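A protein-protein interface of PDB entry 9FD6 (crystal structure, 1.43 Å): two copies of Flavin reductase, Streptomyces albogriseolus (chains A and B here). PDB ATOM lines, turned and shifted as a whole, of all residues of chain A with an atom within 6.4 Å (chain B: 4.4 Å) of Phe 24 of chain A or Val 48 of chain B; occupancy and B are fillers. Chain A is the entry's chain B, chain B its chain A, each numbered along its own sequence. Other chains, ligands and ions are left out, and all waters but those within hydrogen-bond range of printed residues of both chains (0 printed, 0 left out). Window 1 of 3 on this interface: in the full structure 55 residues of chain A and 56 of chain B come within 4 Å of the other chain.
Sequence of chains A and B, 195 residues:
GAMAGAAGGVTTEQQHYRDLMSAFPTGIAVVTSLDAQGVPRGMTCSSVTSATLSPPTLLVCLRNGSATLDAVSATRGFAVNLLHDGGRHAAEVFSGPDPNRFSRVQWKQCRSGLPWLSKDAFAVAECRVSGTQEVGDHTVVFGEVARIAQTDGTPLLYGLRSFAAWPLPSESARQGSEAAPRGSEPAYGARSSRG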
ATOM      1  N   ASP A  19      -0.717   6.234   3.405  1.00  0.00           N
ATOM      2  CA  ASP A  19       0.181   5.119   3.100  1.00  0.00           C
ATOM      3  C   ASP A  19       0.259   4.858   1.599  1.00  0.00           C
ATOM      4  O   ASP A  19       1.330   4.542   1.060  1.00  0.00           O
ATOM      5  CB  ASP A  19      -0.309   3.861   3.827  1.00  0.00           C
ATOM      6  CG  ASP A  19      -0.066   3.905   5.332  1.00  0.00           C
ATOM      7  OD1 ASP A  19       0.693   4.782   5.803  1.00  0.00           O
ATOM      8  OD2 ASP A  19      -0.645   3.055   6.049  1.00  0.00           O
ATOM      9  N   LEU A  20      -0.882   4.962   0.917  1.00  0.00           N
ATOM     10  CA  LEU A  20      -0.915   4.812  -0.531  1.00  0.00           C
ATOM     11  C   LEU A  20      -0.082   5.888  -1.208  1.00  0.00           C
ATOM     12  O   LEU A  20       0.807   5.590  -2.014  1.00  0.00           O
ATOM     13  CB  LEU A  20      -2.362   4.912  -1.010  1.00  0.00           C
ATOM     14  CG  LEU A  20      -2.556   4.967  -2.522  1.00  0.00           C
ATOM     15  CD1 LEU A  20      -2.312   3.599  -3.113  1.00  0.00           C
ATOM     16  CD2 LEU A  20      -3.933   5.481  -2.854  1.00  0.00           C
ATOM     17  N   MET A  21      -0.368   7.153  -0.910  1.00  0.00           N
ATOM     18  CA  MET A  21       0.268   8.229  -1.657  1.00  0.00           C
ATOM     19  C   MET A  21       1.742   8.342  -1.307  1.00  0.00           C
ATOM     20  O   MET A  21       2.540   8.815  -2.124  1.00  0.00           O
ATOM     21  CB  MET A  21      -0.475   9.538  -1.409  1.00  0.00           C
ATOM     22  CG  MET A  21      -1.933   9.500  -1.866  1.00  0.00           C
ATOM     23  SD  MET A  21      -2.176   8.974  -3.577  1.00  0.00           S
ATOM     24  CE  MET A  21      -1.417  10.316  -4.466  1.00  0.00           C
ATOM     25  N   SER A  22       2.128   7.900  -0.105  1.00  0.00           N
ATOM     26  CA  SER A  22       3.543   7.886   0.250  1.00  0.00           C
ATOM     27  C   SER A  22       4.334   6.997  -0.696  1.00  0.00           C
ATOM     28  O   SER A  22       5.531   7.221  -0.909  1.00  0.00           O
ATOM     29  CB  SER A  22       3.725   7.400   1.690  1.00  0.00           C
ATOM     30  OG  SER A  22       3.629   5.985   1.783  1.00  0.00           O
ATOM     31  N   ALA A  23       3.684   5.986  -1.267  1.00  0.00           N
ATOM     32  CA  ALA A  23       4.338   5.021  -2.139  1.00  0.00           C
ATOM     33  C   ALA A  23       4.363   5.439  -3.605  1.00  0.00           C
ATOM     34  O   ALA A  23       4.772   4.636  -4.452  1.00  0.00           O
ATOM     35  CB  ALA A  23       3.685   3.649  -1.962  1.00  0.00           C
ATOM     36  N   PHE A  24       3.964   6.675  -3.917  1.00  0.00           N
ATOM     37  CA  PHE A  24       4.134   7.278  -5.238  1.00  0.00           C
ATOM     38  C   PHE A  24       5.210   8.355  -5.108  1.00  0.00           C
ATOM     39  O   PHE A  24       4.913   9.508  -4.756  1.00  0.00           O
ATOM     40  CB  PHE A  24       2.809   7.866  -5.720  1.00  0.00           C
ATOM     41  CG  PHE A  24       2.830   8.319  -7.148  1.00  0.00           C
ATOM     42  CD1 PHE A  24       2.510   7.462  -8.180  1.00  0.00           C
ATOM     43  CD2 PHE A  24       3.185   9.612  -7.457  1.00  0.00           C
ATOM     44  CE1 PHE A  24       2.540   7.907  -9.497  1.00  0.00           C
ATOM     45  CE2 PHE A  24       3.201  10.055  -8.760  1.00  0.00           C
ATOM     46  CZ  PHE A  24       2.884   9.202  -9.777  1.00  0.00           C
ATOM     47  N   PRO A  25       6.482   8.022  -5.325  1.00  0.00           N
ATOM     48  CA  PRO A  25       7.547   9.010  -5.110  1.00  0.00           C
ATOM     49  C   PRO A  25       7.519  10.098  -6.173  1.00  0.00           C
ATOM     50  O   PRO A  25       6.949   9.938  -7.254  1.00  0.00           O
ATOM     51  CB  PRO A  25       8.837   8.178  -5.185  1.00  0.00           C
ATOM     52  CG  PRO A  25       8.393   6.757  -4.939  1.00  0.00           C
ATOM     53  CD  PRO A  25       7.023   6.674  -5.576  1.00  0.00           C
ATOM     54  N   THR A  26       8.133  11.234  -5.839  1.00  0.00           N
ATOM     55  CA  THR A  26       8.148  12.367  -6.746  1.00  0.00           C
ATOM     56  C   THR A  26       9.458  13.124  -6.602  1.00  0.00           C
ATOM     57  O   THR A  26      10.205  12.941  -5.638  1.00  0.00           O
ATOM     58  CB  THR A  26       7.022  13.370  -6.449  1.00  0.00           C
ATOM     59  OG1 THR A  26       7.228  13.943  -5.151  1.00  0.00           O
ATOM     60  CG2 THR A  26       5.658  12.702  -6.499  1.00  0.00           C
ATOM     61  N   THR A  49       2.644  18.842 -11.307  1.00  0.00           N
ATOM     62  CA  THR A  49       2.090  17.906 -12.277  1.00  0.00           C
ATOM     63  C   THR A  49       1.895  18.613 -13.605  1.00  0.00           C
ATOM     64  O   THR A  49       1.446  19.758 -13.642  1.00  0.00           O
ATOM     65  CB  THR A  49       0.743  17.396 -11.761  1.00  0.00           C
ATOM     66  OG1 THR A  49       0.955  16.748 -10.502  1.00  0.00           O
ATOM     67  CG2 THR A  49       0.097  16.432 -12.734  1.00  0.00           C
ATOM     68  N   TYR A 158      11.448  12.446  -3.108  1.00  0.00           N
ATOM     69  CA  TYR A 158      10.848  12.127  -1.825  1.00  0.00           C
ATOM     70  C   TYR A 158       9.862  10.999  -2.054  1.00  0.00           C
ATOM     71  O   TYR A 158       9.062  11.048  -2.992  1.00  0.00           O
ATOM     72  CB  TYR A 158      10.136  13.329  -1.220  1.00  0.00           C
ATOM     73  CG  TYR A 158       9.797  13.170   0.250  1.00  0.00           C
ATOM     74  CD1 TYR A 158      10.732  13.462   1.230  1.00  0.00           C
ATOM     75  CD2 TYR A 158       8.533  12.765   0.654  1.00  0.00           C
ATOM     76  CE1 TYR A 158      10.431  13.338   2.570  1.00  0.00           C
ATOM     77  CE2 TYR A 158       8.220  12.634   1.995  1.00  0.00           C
ATOM     78  CZ  TYR A 158       9.177  12.933   2.946  1.00  0.00           C
ATOM     79  OH  TYR A 158       8.898  12.820   4.282  1.00  0.00           O
ATOM     80  N   GLY A 159       9.936   9.983  -1.213  1.00  0.00           N
ATOM     81  CA  GLY A 159       9.006   8.881  -1.299  1.00  0.00           C
ATOM     82  C   GLY A 159       9.120   8.041  -0.052  1.00  0.00           C
ATOM     83  O   GLY A 159      10.186   7.996   0.571  1.00  0.00           O
ATOM     84  N   LEU A 160       8.031   7.385   0.329  1.00  0.00           N
ATOM     85  CA  LEU A 160       8.042   6.518   1.497  1.00  0.00           C
ATOM     86  C   LEU A 160       8.678   7.253   2.675  1.00  0.00           C
ATOM     87  O   LEU A 160       9.534   6.731   3.392  1.00  0.00           O
ATOM     88  CB  LEU A 160       8.742   5.199   1.179  1.00  0.00           C
ATOM     89  CG  LEU A 160       8.049   4.394   0.070  1.00  0.00           C
ATOM     90  CD1 LEU A 160       8.918   3.225  -0.382  1.00  0.00           C
ATOM     91  CD2 LEU A 160       6.669   3.916   0.537  1.00  0.00           C
ATOM     92  N   THR B  26       8.630  10.681 -11.211  1.00  0.00           N
ATOM     93  CA  THR B  26       7.441  10.246 -10.507  1.00  0.00           C
ATOM     94  C   THR B  26       7.406   8.725 -10.432  1.00  0.00           C
ATOM     95  O   THR B  26       8.126   8.021 -11.144  1.00  0.00           O
ATOM     96  CB  THR B  26       6.163  10.693 -11.228  1.00  0.00           C
ATOM     97  OG1 THR B  26       6.090  10.021 -12.491  1.00  0.00           O
ATOM     98  CG2 THR B  26       6.145  12.198 -11.466  1.00  0.00           C
ATOM     99  N   GLY B  27       6.541   8.226  -9.560  1.00  0.00           N
ATOM    100  CA  GLY B  27       6.085   6.859  -9.679  1.00  0.00           C
ATOM    101  C   GLY B  27       5.287   6.664 -10.955  1.00  0.00           C
ATOM    102  O   GLY B  27       5.101   7.598 -11.747  1.00  0.00           O
ATOM    103  N   ILE B  28       4.796   5.453 -11.172  1.00  0.00           N
ATOM    104  CA  ILE B  28       4.040   5.144 -12.374  1.00  0.00           C
ATOM    105  C   ILE B  28       2.810   4.356 -11.976  1.00  0.00           C
ATOM    106  O   ILE B  28       2.914   3.344 -11.271  1.00  0.00           O
ATOM    107  CB  ILE B  28       4.872   4.344 -13.392  1.00  0.00           C
ATOM    108  CG1 ILE B  28       5.929   5.234 -14.031  1.00  0.00           C
ATOM    109  CG2 ILE B  28       3.956   3.756 -14.448  1.00  0.00           C
ATOM    110  CD1 ILE B  28       5.389   6.281 -14.988  1.00  0.00           C
ATOM    111  N   ALA B  29       1.654   4.806 -12.441  1.00  0.00           N
ATOM    112  CA  ALA B  29       0.424   4.062 -12.269  1.00  0.00           C
ATOM    113  C   ALA B  29      -0.123   3.648 -13.627  1.00  0.00           C
ATOM    114  O   ALA B  29       0.239   4.198 -14.670  1.00  0.00           O
ATOM    115  CB  ALA B  29      -0.633   4.900 -11.544  1.00  0.00           C
ATOM    116  N   CYS B  45      -0.002   6.314 -16.412  1.00  0.00           N
ATOM    117  CA  CYS B  45      -0.283   7.635 -15.874  1.00  0.00           C
ATOM    118  C   CYS B  45       0.799   7.995 -14.873  1.00  0.00           C
ATOM    119  O   CYS B  45       1.043   7.254 -13.916  1.00  0.00           O
ATOM    120  CB  CYS B  45      -1.649   7.624 -15.190  1.00  0.00           C
ATOM    121  SG  CYS B  45      -2.119   9.156 -14.476  1.00  0.00           S
ATOM    122  N   SER B  46       1.447   9.130 -15.112  1.00  0.00           N
ATOM    123  CA  SER B  46       2.435   9.687 -14.206  1.00  0.00           C
ATOM    124  C   SER B  46       1.918  10.917 -13.476  1.00  0.00           C
ATOM    125  O   SER B  46       2.662  11.512 -12.696  1.00  0.00           O
ATOM    126  CB  SER B  46       3.708  10.042 -14.988  1.00  0.00           C
ATOM    127  OG  SER B  46       3.425  10.948 -16.037  1.00  0.00           O
ATOM    128  N   SER B  47       0.658  11.302 -13.687  1.00  0.00           N
ATOM    129  CA  SER B  47       0.114  12.544 -13.147  1.00  0.00           C
ATOM    130  C   SER B  47      -0.680  12.343 -11.853  1.00  0.00           C
ATOM    131  O   SER B  47      -1.467  13.215 -11.466  1.00  0.00           O
ATOM    132  CB  SER B  47      -0.744  13.240 -14.208  1.00  0.00           C
ATOM    133  OG  SER B  47      -1.756  12.370 -14.695  1.00  0.00           O
ATOM    134  N   VAL B  48      -0.500  11.209 -11.180  1.00  0.00           N
ATOM    135  CA  VAL B  48      -1.185  10.979  -9.916  1.00  0.00           C
ATOM    136  C   VAL B  48      -0.677  11.976  -8.886  1.00  0.00           C
ATOM    137  O   VAL B  48       0.530  12.079  -8.639  1.00  0.00           O
ATOM    138  CB  VAL B  48      -0.947   9.539  -9.444  1.00  0.00           C
ATOM    139  CG1 VAL B  48      -1.633   9.305  -8.104  1.00  0.00           C
ATOM    140  CG2 VAL B  48      -1.431   8.553 -10.483  1.00  0.00           C
ATOM    141  N   THR B  49      -1.597  12.698  -8.257  1.00  0.00           N
ATOM    142  CA  THR B  49      -1.236  13.773  -7.346  1.00  0.00           C
ATOM    143  C   THR B  49      -2.206  13.787  -6.181  1.00  0.00           C
ATOM    144  O   THR B  49      -3.409  13.607  -6.366  1.00  0.00           O
ATOM    145  CB  THR B  49      -1.302  15.111  -8.094  1.00  0.00           C
ATOM    146  OG1 THR B  49      -0.448  15.055  -9.244  1.00  0.00           O
ATOM    147  CG2 THR B  49      -0.895  16.251  -7.195  1.00  0.00           C
ATOM    148  N   LEU B  59      -5.859  13.318  -7.722  1.00  0.00           N
ATOM    149  CA  LEU B  59      -6.212  13.716  -9.073  1.00  0.00           C
ATOM    150  C   LEU B  59      -5.276  13.033 -10.057  1.00  0.00           C
ATOM    151  O   LEU B  59      -4.165  12.608  -9.717  1.00  0.00           O
ATOM    152  CB  LEU B  59      -6.209  15.241  -9.243  1.00  0.00           C
ATOM    153  CG  LEU B  59      -4.881  15.967  -9.085  1.00  0.00           C
ATOM    154  CD1 LEU B  59      -4.043  15.865 -10.367  1.00  0.00           C
ATOM    155  CD2 LEU B  59      -5.118  17.420  -8.731  1.00  0.00           C
ATOM    156  N   VAL B  60      -5.777  12.900 -11.281  1.00  0.00           N
ATOM    157  CA  VAL B  60      -5.000  12.456 -12.427  1.00  0.00           C
ATOM    158  C   VAL B  60      -5.326  13.406 -13.568  1.00  0.00           C
ATOM    159  O   VAL B  60      -6.367  14.069 -13.575  1.00  0.00           O
ATOM    160  CB  VAL B  60      -5.264  10.979 -12.801  1.00  0.00           C
ATOM    161  CG1 VAL B  60      -4.831  10.083 -11.655  1.00  0.00           C
ATOM    162  CG2 VAL B  60      -6.721  10.735 -13.151  1.00  0.00           C
ATOM    163  N   VAL B  80      -6.577   3.268  -9.662  1.00  0.00           N
ATOM    164  CA  VAL B  80      -5.190   3.693  -9.765  1.00  0.00           C
ATOM    165  C   VAL B  80      -4.343   2.513  -9.304  1.00  0.00           C
ATOM    166  O   VAL B  80      -4.386   2.133  -8.128  1.00  0.00           O
ATOM    167  CB  VAL B  80      -4.921   4.949  -8.927  1.00  0.00           C
ATOM    168  CG1 VAL B  80      -3.447   5.307  -9.010  1.00  0.00           C
ATOM    169  CG2 VAL B  80      -5.807   6.104  -9.397  1.00  0.00           C
ATOM    170  N   LEU B  82      -0.739   1.278  -8.705  1.00  0.00           N
ATOM    171  CA  LEU B  82       0.647   1.715  -8.559  1.00  0.00           C
ATOM    172  C   LEU B  82       1.590   0.565  -8.901  1.00  0.00           C
ATOM    173  O   LEU B  82       1.547  -0.496  -8.268  1.00  0.00           O
ATOM    174  CB  LEU B  82       0.922   2.218  -7.143  1.00  0.00           C
ATOM    175  CG  LEU B  82       0.054   3.373  -6.638  1.00  0.00           C
ATOM    176  CD1 LEU B  82       0.575   3.856  -5.284  1.00  0.00           C
ATOM    177  CD2 LEU B  82       0.008   4.494  -7.670  1.00  0.00           C
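The backbone NH of Gly 27 of chain B is in hydrogen-bond range of the backbone carbonyl oxygen of Pro 25 of chain A (2.9 Å).
The side-chain hydroxyl of Thr 49 of chain B is in hydrogen-bond range of the side-chain hydroxyl of Thr 49 of chain A, at 2.5 Å.
O of Thr 49 of chain B sits at hydrogen-bond distance from N of Leu 59 of chain B.
The side-chain hydroxyl (OG) of Ser 47 of chain B is in hydrogen-bond range of the side-chain sulfur (SG) of Cys 45 of chain B, at 3.2 Å.
OG1 of Thr 49 of chain B is in hydrogen-bond range of O of Ser 47 of chain B (3.1 Å).
CD1 of Leu 82 of chain B touches CD1 of Leu 20 of chain A, 3.6 Å away.
Val 48 of chain B touches Met 21 of chain A.
Thr 49 of chain B touches Met 21 of chain A.
Phe 24 of chain A touches Thr 26 of chain B (CZ to CB, 3.9 Å).
Phe 24 of chain A touches Gly 27 of chain B (CE1 to C, 3.3 Å).
Ile 28 of chain B touches Phe 24 of chain A.
Phe 24 of chain A touches Ser 46 of chain B.
O of Val 48 of chain B touches CE2 of Phe 24 of chain A, at 3.4 Å.
Phe 24 of chain A touches Leu 82 of chain B.
Pro 25 of chain A touches Thr 26 of chain B.
Of chain B, only Thr 26, Gly 27, Ile 28, Ser 46, Val 48 and Leu 82 come within 4 Å of Phe 24 of chain A.
Val 48 of chain B touches two residues of chain A.
Of the printed residues of chain B, Pro 25 of chain A touches Thr 26 and Gly 27.
Printed residues of chain A within 4 Å of Thr 49 of chain B: Met 21 (3.95 Å) and Thr 49 (2.5 Å).
Of the printed residues of chain A, Ser 46 of chain B touches Phe 24 (3.7 Å).
Printed residues of chain A within 4 Å of Ser 47 of chain B: Thr 49.
Ala 29 of chain B touches none of the printed residues of chain A.
The nearest printed residue of chain B that does not touch Phe 24 of chain A is Ala 29 of chain B (4.4 Å).
Hydrophobic or aromatic side chains of chain A that line the printed part of chain B: Leu 20, Met 21 and Phe 24.
Of the 13 printed residues of chain B, 8 touch a printed residue of chain A.
Along chain B the printed residues that touch a printed residue of chain A span positions 26 to 82.
Among the printed residues, 13 pairs touch across the chains.
Among the printed residues, no Asp or Glu carboxylate lies within 4 Å of a Lys or Arg side-chain nitrogen of the other chain.
Thr 49 of chain B touches its own counterpart, Thr 49 of chain A.
Of the 13 pairs that touch across the chains among the printed residues, 1 has its exchanged pair printed and touching as well.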
